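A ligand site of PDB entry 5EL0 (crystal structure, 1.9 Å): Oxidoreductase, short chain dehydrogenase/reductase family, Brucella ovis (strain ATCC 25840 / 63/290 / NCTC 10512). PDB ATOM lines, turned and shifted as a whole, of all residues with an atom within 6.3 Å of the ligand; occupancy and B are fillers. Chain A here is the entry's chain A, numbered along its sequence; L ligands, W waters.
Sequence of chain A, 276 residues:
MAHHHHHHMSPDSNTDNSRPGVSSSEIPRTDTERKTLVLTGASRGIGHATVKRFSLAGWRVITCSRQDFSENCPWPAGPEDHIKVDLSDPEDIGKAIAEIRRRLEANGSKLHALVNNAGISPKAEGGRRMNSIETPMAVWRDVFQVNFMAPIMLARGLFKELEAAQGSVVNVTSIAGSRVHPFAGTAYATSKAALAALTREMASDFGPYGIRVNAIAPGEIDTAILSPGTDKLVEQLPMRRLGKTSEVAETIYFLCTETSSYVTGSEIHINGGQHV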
ATOM      1  N   THR A  40      -1.676   6.814  10.173  1.00  0.00           N
ATOM      2  CA  THR A  40      -1.226   6.409  11.499  1.00  0.00           C
ATOM      3  C   THR A  40      -0.260   7.451  12.041  1.00  0.00           C
ATOM      4  O   THR A  40       0.362   8.200  11.268  1.00  0.00           O
ATOM      5  CB  THR A  40      -0.558   5.021  11.473  1.00  0.00           C
ATOM      6  OG1 THR A  40       0.738   5.115  10.860  1.00  0.00           O
ATOM      7  CG2 THR A  40      -1.421   4.033  10.683  1.00  0.00           C
ATOM      8  N   GLY A  41      -0.142   7.509  13.357  1.00  0.00           N
ATOM      9  CA  GLY A  41       0.810   8.441  13.942  1.00  0.00           C
ATOM     10  C   GLY A  41       0.393   9.887  13.760  1.00  0.00           C
ATOM     11  O   GLY A  41       1.187  10.737  13.349  1.00  0.00           O
ATOM     12  N   ALA A  42      -0.869  10.174  14.081  1.00  0.00           N
ATOM     13  CA  ALA A  42      -1.386  11.546  14.006  1.00  0.00           C
ATOM     14  C   ALA A  42      -1.066  12.315  15.286  1.00  0.00           C
ATOM     15  O   ALA A  42      -1.936  12.827  15.996  1.00  0.00           O
ATOM     16  CB  ALA A  42      -2.888  11.509  13.745  1.00  0.00           C
ATOM     17  N   SER A  43       0.237  12.401  15.585  1.00  0.00           N
ATOM     18  CA  SER A  43       0.776  13.029  16.781  1.00  0.00           C
ATOM     19  C   SER A  43       1.162  14.479  16.509  1.00  0.00           C
ATOM     20  O   SER A  43       1.255  14.909  15.360  1.00  0.00           O
ATOM     21  CB  SER A  43       1.991  12.247  17.284  1.00  0.00           C
ATOM     22  OG  SER A  43       2.798  11.862  16.178  1.00  0.00           O
ATOM     23  N   ARG A  44       1.409  15.224  17.589  1.00  0.00           N
ATOM     24  CA  ARG A  44       1.792  16.629  17.440  1.00  0.00           C
ATOM     25  C   ARG A  44       3.025  16.731  16.548  1.00  0.00           C
ATOM     26  O   ARG A  44       3.905  15.854  16.559  1.00  0.00           O
ATOM     27  CB  ARG A  44       2.062  17.265  18.811  1.00  0.00           C
ATOM     28  N   CYS A  64      -5.798   6.714  12.865  1.00  0.00           N
ATOM     29  CA  CYS A  64      -5.675   5.532  13.702  1.00  0.00           C
ATOM     30  C   CYS A  64      -4.921   5.898  14.976  1.00  0.00           C
ATOM     31  O   CYS A  64      -3.894   6.573  14.913  1.00  0.00           O
ATOM     32  CB  CYS A  64      -4.943   4.419  12.963  1.00  0.00           C
ATOM     33  SG  CYS A  64      -5.705   3.980  11.391  1.00  0.00           S
ATOM     34  N   SER A  65      -5.436   5.461  16.119  1.00  0.00           N
ATOM     35  CA  SER A  65      -4.836   5.829  17.390  1.00  0.00           C
ATOM     36  C   SER A  65      -5.203   4.758  18.407  1.00  0.00           C
ATOM     37  O   SER A  65      -6.213   4.078  18.253  1.00  0.00           O
ATOM     38  CB  SER A  65      -5.318   7.220  17.843  1.00  0.00           C
ATOM     39  OG  SER A  65      -5.366   7.321  19.242  1.00  0.00           O
ATOM     40  N   ARG A  66      -4.376   4.623  19.453  1.00  0.00           N
ATOM     41  CA  ARG A  66      -4.735   3.708  20.525  1.00  0.00           C
ATOM     42  C   ARG A  66      -5.866   4.250  21.389  1.00  0.00           C
ATOM     43  O   ARG A  66      -6.482   3.472  22.135  1.00  0.00           O
ATOM     44  CB  ARG A  66      -3.528   3.440  21.422  1.00  0.00           C
ATOM     45  CG  ARG A  66      -2.510   2.524  20.782  1.00  0.00           C
ATOM     46  CD  ARG A  66      -1.171   2.628  21.505  1.00  0.00           C
ATOM     47  NE  ARG A  66      -0.667   3.999  21.541  1.00  0.00           N
ATOM     48  CZ  ARG A  66       0.532   4.336  21.978  1.00  0.00           C
ATOM     49  NH1 ARG A  66       1.366   3.398  22.423  1.00  0.00           N
ATOM     50  NH2 ARG A  66       0.918   5.611  21.974  1.00  0.00           N
ATOM     51  N   GLN A  67      -6.158   5.535  21.292  1.00  0.00           N
ATOM     52  CA  GLN A  67      -7.088   6.191  22.208  1.00  0.00           C
ATOM     53  C   GLN A  67      -8.508   6.112  21.680  1.00  0.00           C
ATOM     54  O   GLN A  67      -8.739   5.977  20.470  1.00  0.00           O
ATOM     55  CB  GLN A  67      -6.684   7.654  22.406  1.00  0.00           C
ATOM     56  N   VAL A  85      -6.968   1.526  17.363  1.00  0.00           N
ATOM     57  CA  VAL A  85      -6.205   0.331  17.039  1.00  0.00           C
ATOM     58  C   VAL A  85      -4.851   0.426  17.731  1.00  0.00           C
ATOM     59  O   VAL A  85      -4.235   1.495  17.792  1.00  0.00           O
ATOM     60  CB  VAL A  85      -6.050   0.148  15.512  1.00  0.00           C
ATOM     61  CG1 VAL A  85      -5.413   1.377  14.889  1.00  0.00           C
ATOM     62  CG2 VAL A  85      -5.206  -1.110  15.199  1.00  0.00           C
ATOM     63  N   ASP A  86      -4.424  -0.702  18.285  1.00  0.00           N
ATOM     64  CA  ASP A  86      -3.083  -0.829  18.829  1.00  0.00           C
ATOM     65  C   ASP A  86      -2.225  -1.528  17.764  1.00  0.00           C
ATOM     66  O   ASP A  86      -2.384  -2.721  17.529  1.00  0.00           O
ATOM     67  CB  ASP A  86      -3.100  -1.618  20.134  1.00  0.00           C
ATOM     68  CG  ASP A  86      -1.740  -1.707  20.790  1.00  0.00           C
ATOM     69  OD1 ASP A  86      -0.708  -1.501  20.117  1.00  0.00           O
ATOM     70  OD2 ASP A  86      -1.693  -2.013  21.997  1.00  0.00           O
ATOM     71  N   LEU A  87      -1.312  -0.765  17.142  1.00  0.00           N
ATOM     72  CA  LEU A  87      -0.506  -1.291  16.057  1.00  0.00           C
ATOM     73  C   LEU A  87       0.549  -2.289  16.525  1.00  0.00           C
ATOM     74  O   LEU A  87       1.232  -2.877  15.677  1.00  0.00           O
ATOM     75  CB  LEU A  87       0.163  -0.136  15.296  1.00  0.00           C
ATOM     76  CG  LEU A  87      -0.805   0.850  14.634  1.00  0.00           C
ATOM     77  CD1 LEU A  87      -0.036   2.012  13.993  1.00  0.00           C
ATOM     78  CD2 LEU A  87      -1.692   0.136  13.611  1.00  0.00           C
ATOM     79  N   SER A  88       0.709  -2.466  17.839  1.00  0.00           N
ATOM     80  CA  SER A  88       1.580  -3.550  18.301  1.00  0.00           C
ATOM     81  C   SER A  88       0.855  -4.890  18.351  1.00  0.00           C
ATOM     82  O   SER A  88       1.458  -5.876  18.771  1.00  0.00           O
ATOM     83  CB  SER A  88       2.148  -3.232  19.681  1.00  0.00           C
ATOM     84  OG  SER A  88       1.139  -3.333  20.664  1.00  0.00           O
ATOM     85  N   ASP A  89      -0.427  -4.933  17.979  1.00  0.00           N
ATOM     86  CA  ASP A  89      -1.251  -6.134  18.155  1.00  0.00           C
ATOM     87  C   ASP A  89      -1.757  -6.584  16.799  1.00  0.00           C
ATOM     88  O   ASP A  89      -2.636  -5.911  16.216  1.00  0.00           O
ATOM     89  CB  ASP A  89      -2.409  -5.813  19.122  1.00  0.00           C
ATOM     90  CG  ASP A  89      -3.282  -7.017  19.442  1.00  0.00           C
ATOM     91  OD1 ASP A  89      -3.474  -7.882  18.566  1.00  0.00           O
ATOM     92  OD2 ASP A  89      -3.803  -7.081  20.563  1.00  0.00           O
ATOM     93  N   ASN A 117       2.885   6.982   9.698  1.00  0.00           N
ATOM     94  CA  ASN A 117       3.734   7.855  10.507  1.00  0.00           C
ATOM     95  C   ASN A 117       3.864   7.390  11.953  1.00  0.00           C
ATOM     96  O   ASN A 117       4.635   8.002  12.703  1.00  0.00           O
ATOM     97  CB  ASN A 117       3.190   9.298  10.499  1.00  0.00           C
ATOM     98  CG  ASN A 117       4.180  10.290  11.115  1.00  0.00           C
ATOM     99  OD1 ASN A 117       5.342  10.357  10.714  1.00  0.00           O
ATOM    100  ND2 ASN A 117       3.731  11.033  12.126  1.00  0.00           N
ATOM    101  N   ALA A 118       3.160   6.350  12.367  1.00  0.00           N
ATOM    102  CA  ALA A 118       3.296   5.873  13.736  1.00  0.00           C
ATOM    103  C   ALA A 118       4.720   5.388  13.971  1.00  0.00           C
ATOM    104  O   ALA A 118       5.326   4.758  13.108  1.00  0.00           O
ATOM    105  CB  ALA A 118       2.299   4.745  14.021  1.00  0.00           C
ATOM    106  N   GLY A 119       5.282   5.708  15.135  1.00  0.00           N
ATOM    107  CA  GLY A 119       6.606   5.204  15.429  1.00  0.00           C
ATOM    108  C   GLY A 119       6.841   5.303  16.920  1.00  0.00           C
ATOM    109  O   GLY A 119       6.382   6.260  17.557  1.00  0.00           O
ATOM    110  N   ILE A 120       7.533   4.324  17.501  1.00  0.00           N
ATOM    111  CA  ILE A 120       7.842   4.339  18.920  1.00  0.00           C
ATOM    112  C   ILE A 120       9.335   4.132  19.117  1.00  0.00           C
ATOM    113  O   ILE A 120      10.004   3.464  18.310  1.00  0.00           O
ATOM    114  CB  ILE A 120       7.045   3.265  19.700  1.00  0.00           C
ATOM    115  CG1 ILE A 120       7.194   1.881  19.078  1.00  0.00           C
ATOM    116  CG2 ILE A 120       5.573   3.674  19.811  1.00  0.00           C
ATOM    117  CD1 ILE A 120       6.733   0.790  20.037  1.00  0.00           C
ATOM    118  N   SER A 121       9.854   4.692  20.203  1.00  0.00           N
ATOM    119  CA  SER A 121      11.248   4.499  20.620  1.00  0.00           C
ATOM    120  C   SER A 121      11.276   4.435  22.142  1.00  0.00           C
ATOM    121  O   SER A 121      11.568   5.440  22.824  1.00  0.00           O
ATOM    122  CB  SER A 121      12.151   5.620  20.097  1.00  0.00           C
ATOM    123  OG  SER A 121      13.497   5.435  20.495  1.00  0.00           O
ATOM    124  N   LYS A 123      12.193   4.075  26.017  1.00  0.00           N
ATOM    125  CA  LYS A 123      13.380   4.499  26.731  1.00  0.00           C
ATOM    126  C   LYS A 123      13.724   3.527  27.848  1.00  0.00           C
ATOM    127  O   LYS A 123      12.847   2.835  28.369  1.00  0.00           O
ATOM    128  CB  LYS A 123      13.200   5.911  27.300  1.00  0.00           C
ATOM    129  CG  LYS A 123      12.847   6.927  26.222  1.00  0.00           C
ATOM    130  CD  LYS A 123      13.483   8.270  26.512  1.00  0.00           C
ATOM    131  CE  LYS A 123      12.564   9.433  26.177  1.00  0.00           C
ATOM    132  NZ  LYS A 123      11.806   9.937  27.372  1.00  0.00           N
ATOM    133  N   VAL A 146       5.320  -2.136  15.477  1.00  0.00           N
ATOM    134  CA  VAL A 146       4.653  -0.854  15.214  1.00  0.00           C
ATOM    135  C   VAL A 146       5.301  -0.136  14.028  1.00  0.00           C
ATOM    136  O   VAL A 146       4.619   0.367  13.133  1.00  0.00           O
ATOM    137  CB  VAL A 146       4.659   0.031  16.479  1.00  0.00           C
ATOM    138  CG1 VAL A 146       4.158   1.453  16.157  1.00  0.00           C
ATOM    139  CG2 VAL A 146       3.808  -0.592  17.592  1.00  0.00           C
ATOM    140  N   THR A 223       9.831  14.750  16.934  1.00  0.00           N
ATOM    141  CA  THR A 223       9.726  14.998  18.370  1.00  0.00           C
ATOM    142  C   THR A 223       8.654  14.154  19.032  1.00  0.00           C
ATOM    143  O   THR A 223       8.629  14.059  20.276  1.00  0.00           O
ATOM    144  CB  THR A 223       9.452  16.480  18.645  1.00  0.00           C
ATOM    145  OG1 THR A 223       8.292  16.892  17.915  1.00  0.00           O
ATOM    146  CG2 THR A 223      10.641  17.324  18.217  1.00  0.00           C
ATOM    147  N   ALA A 224       7.780  13.538  18.250  1.00  0.00           N
ATOM    148  CA  ALA A 224       6.807  12.626  18.827  1.00  0.00           C
ATOM    149  C   ALA A 224       7.462  11.489  19.606  1.00  0.00           C
ATOM    150  O   ALA A 224       6.850  10.977  20.540  1.00  0.00           O
ATOM    151  CB  ALA A 224       5.886  12.067  17.746  1.00  0.00           C
ATOM    152  N   ILE A 225       8.694  11.085  19.288  1.00  0.00           N
ATOM    153  CA  ILE A 225       9.293   9.960  20.026  1.00  0.00           C
ATOM    154  C   ILE A 225      10.004  10.412  21.301  1.00  0.00           C
ATOM    155  O   ILE A 225      10.527   9.569  22.044  1.00  0.00           O
ATOM    156  CB  ILE A 225      10.272   9.120  19.188  1.00  0.00           C
ATOM    157  CG1 ILE A 225      11.532   9.907  18.854  1.00  0.00           C
ATOM    158  CG2 ILE A 225       9.588   8.592  17.927  1.00  0.00           C
ATOM    159  CD1 ILE A 225      12.621   9.040  18.265  1.00  0.00           C
ATOM    160  N   LEU A 226      10.032  11.707  21.592  1.00  0.00           N
ATOM    161  CA  LEU A 226      10.722  12.195  22.779  1.00  0.00           C
ATOM    162  C   LEU A 226       9.967  11.813  24.052  1.00  0.00           C
ATOM    163  O   LEU A 226       8.746  11.935  24.126  1.00  0.00           O
ATOM    164  CB  LEU A 226      10.891  13.717  22.712  1.00  0.00           C
HETATM  165  P1  LIG L   1       3.532   8.389  21.244  1.00  0.00           P
HETATM  166  O1  LIG L   1       2.244   9.119  21.370  1.00  0.00           O
HETATM  167  O2  LIG L   1       3.533   7.233  22.222  1.00  0.00           O
HETATM  168  O3  LIG L   1       3.581   7.690  19.723  1.00  0.00           O
HETATM  169  C1  LIG L   1       3.877   8.482  18.563  1.00  0.00           C
HETATM  170  C2  LIG L   1       2.753   8.384  17.561  1.00  0.00           C
HETATM  171  O4  LIG L   1       2.622   7.021  17.098  1.00  0.00           O
HETATM  172  C3  LIG L   1       1.380   8.793  18.100  1.00  0.00           C
HETATM  173  O5  LIG L   1       0.591   9.438  17.100  1.00  0.00           O
HETATM  174  C4  LIG L   1       0.745   7.456  18.451  1.00  0.00           C
HETATM  175  O6  LIG L   1      -0.697   7.438  18.409  1.00  0.00           O
HETATM  176  C5  LIG L   1       1.334   6.519  17.398  1.00  0.00           C
HETATM  177  N1  LIG L   1       1.470   5.164  17.886  1.00  0.00           N
HETATM  178  C6  LIG L   1       2.511   4.676  18.630  1.00  0.00           C
HETATM  179  N2  LIG L   1       2.343   3.447  19.051  1.00  0.00           N
HETATM  180  C7  LIG L   1       1.107   3.091  18.522  1.00  0.00           C
HETATM  181  C8  LIG L   1       0.352   1.912  18.613  1.00  0.00           C
HETATM  182  N3  LIG L   1       0.755   0.827  19.296  1.00  0.00           N
HETATM  183  N4  LIG L   1      -0.855   1.893  18.003  1.00  0.00           N
HETATM  184  C9  LIG L   1      -1.258   2.984  17.344  1.00  0.00           C
HETATM  185  N5  LIG L   1      -0.622   4.151  17.181  1.00  0.00           N
HETATM  186  C10 LIG L   1       0.557   4.141  17.802  1.00  0.00           C
HETATM  187  O7  LIG L   1       4.716   9.393  21.617  1.00  0.00           O
HETATM  188  P2  LIG L   1       4.747  10.776  22.428  1.00  0.00           P
HETATM  189  O8  LIG L   1       4.647  11.893  21.472  1.00  0.00           O
HETATM  190  O9  LIG L   1       3.764  10.717  23.536  1.00  0.00           O
HETATM  191  O10 LIG L   1       6.219  10.783  23.031  1.00  0.00           O
HETATM  192  C11 LIG L   1       6.790   9.564  23.536  1.00  0.00           C
HETATM  193  C12 LIG L   1       6.693   9.532  25.043  1.00  0.00           C
HETATM  194  O11 LIG L   1       5.309   9.598  25.446  1.00  0.00           O
HETATM  195  C13 LIG L   1       7.255   8.275  25.707  1.00  0.00           C
HETATM  196  O12 LIG L   1       7.796   8.556  26.986  1.00  0.00           O
HETATM  197  C14 LIG L   1       6.029   7.371  25.771  1.00  0.00           C
HETATM  198  O13 LIG L   1       6.124   6.454  26.851  1.00  0.00           O
HETATM  199  C15 LIG L   1       4.908   8.376  26.021  1.00  0.00           C
HETATM  200  P3  LIG L   1      -1.639   7.328  19.747  1.00  0.00           P
HETATM  201  O14 LIG L   1      -2.818   8.254  19.575  1.00  0.00           O
HETATM  202  O15 LIG L   1      -2.047   5.868  19.846  1.00  0.00           O
HETATM  203  O16 LIG L   1      -0.738   7.671  20.943  1.00  0.00           O
HETATM  204  O   HOH W   1       9.821   7.378  24.001  1.00  0.00           O
HETATM  205  O   HOH W   2       4.568   9.431  14.963  1.00  0.00           O
HETATM  206  O   HOH W   3      -2.407   8.647  15.823  1.00  0.00           O
HETATM  207  O   HOH W   4      -1.880  10.404  18.147  1.00  0.00           O
HETATM  208  O   HOH W   5       4.113   4.899  23.404  1.00  0.00           O
HETATM  209  O   HOH W   6       3.073   1.021  21.120  1.00  0.00           O
HETATM  210  O   HOH W   7      -1.296   5.543  14.973  1.00  0.00           O
HETATM  211  O   HOH W   8       7.437   3.428  26.032  1.00  0.00           O
HETATM  212  O   HOH W   9       7.509  12.539  26.361  1.00  0.00           O
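O of Ala 224 lies close to O8 of the ligand.
The backbone NH (N) of Arg 66 sits at hydrogen-bond distance from an oxygen (O15) of the ligand, 2.7 Å away.
O16 of the ligand lies within salt-bridge range of NH2 of Arg 66, at 2.8 Å.
OG of Ser 65 is in hydrogen-bond range of O14 of the ligand, at 2.7 Å.
N4 of the ligand sits at hydrogen-bond distance from N of Leu 87 (2.8 Å).
OD1 of Asp 86 lies within hydrogen-bond range of N3 of the ligand.
The backbone NH (N) of Ser 43 sits close to an oxygen (O5) of the ligand (3.3 Å).
OG of Ser 43 sits close to O5 of the ligand, at 3.4 Å.
An oxygen (O5) of the ligand lies within hydrogen-bond range of the backbone NH (N) of Ala 42 (3.4 Å).
The backbone carbonyl oxygen of Ser 65 sits at hydrogen-bond distance from the backbone NH of Val 85 (2.8 Å).
The side-chain hydroxyl (OG) of Ser 65 lies within hydrogen-bond range of the backbone NH (N) of Gln 67, at 2.8 Å.
The side-chain hydroxyl (OG) of Ser 88 lies within hydrogen-bond range of the side-chain carboxylate (OD1) of Asp 86, 2.7 Å away.
OG of Ser 43 lies within hydrogen-bond range of O of Gly 41, 3.4 Å away.
ND2 of Asn 117 lies within hydrogen-bond range of O of Gly 41 (2.8 Å).
The backbone NH of Ala 118 lies within hydrogen-bond range of the side-chain hydroxyl of Thr 40, 3.1 Å away.
The backbone carbonyl oxygen (O) of Val 85 lies close to a nitrogen (N4) of the ligand (3.4 Å).
The backbone carbonyl oxygen (O) of Leu 226 sits close to an oxygen (O10) of the ligand (3.0 Å).
CA of Gly 41 touches O5 of the ligand, 3.3 Å away.
N of Ser 88 touches N3 of the ligand, 3.6 Å away.
CA of Ala 118 touches O4 of the ligand, at 3.6 Å.
Gly 119 touches the ligand (O to C1, 3.5 Å).
Ile 120 touches the ligand (CG2 to N2, 3.3 Å).
CG2 of Val 146 touches N3 of the ligand, at 3.8 Å.
Hydrophobic or aromatic side chains that line the ligand: Leu 87, Ala 118, Ile 120, Val 146 and Ala 224.
The nearest printed residue that does not touch the ligand is Ile 225 (4.01 Å).
Water W5 lies within hydrogen-bond range of O2 of the ligand (2.7 Å) and NH1 of Arg 66 (3.3 Å).
Water W7 lies within hydrogen-bond range of a nitrogen (N5) of the ligand (2.7 Å), the backbone NH of Gly 41 (2.8 Å) and the backbone carbonyl oxygen of Cys 64 (2.8 Å).
Water W4 bridges an oxygen (O14) of the ligand and the backbone carbonyl oxygen (O) of Ala 42.
Water W1 bridges the backbone carbonyl oxygen (O) of Ser 121 and the backbone carbonyl oxygen (O) of Ile 225.
Water W3 lies within hydrogen-bond range of O of Cys 64 (2.7 Å), N of Ala 42 (2.8 Å) and O6 of the ligand (3.3 Å).
Water W2 bridges O of Asn 117 (2.7 Å) and OG of Ser 43 (3.2 Å).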
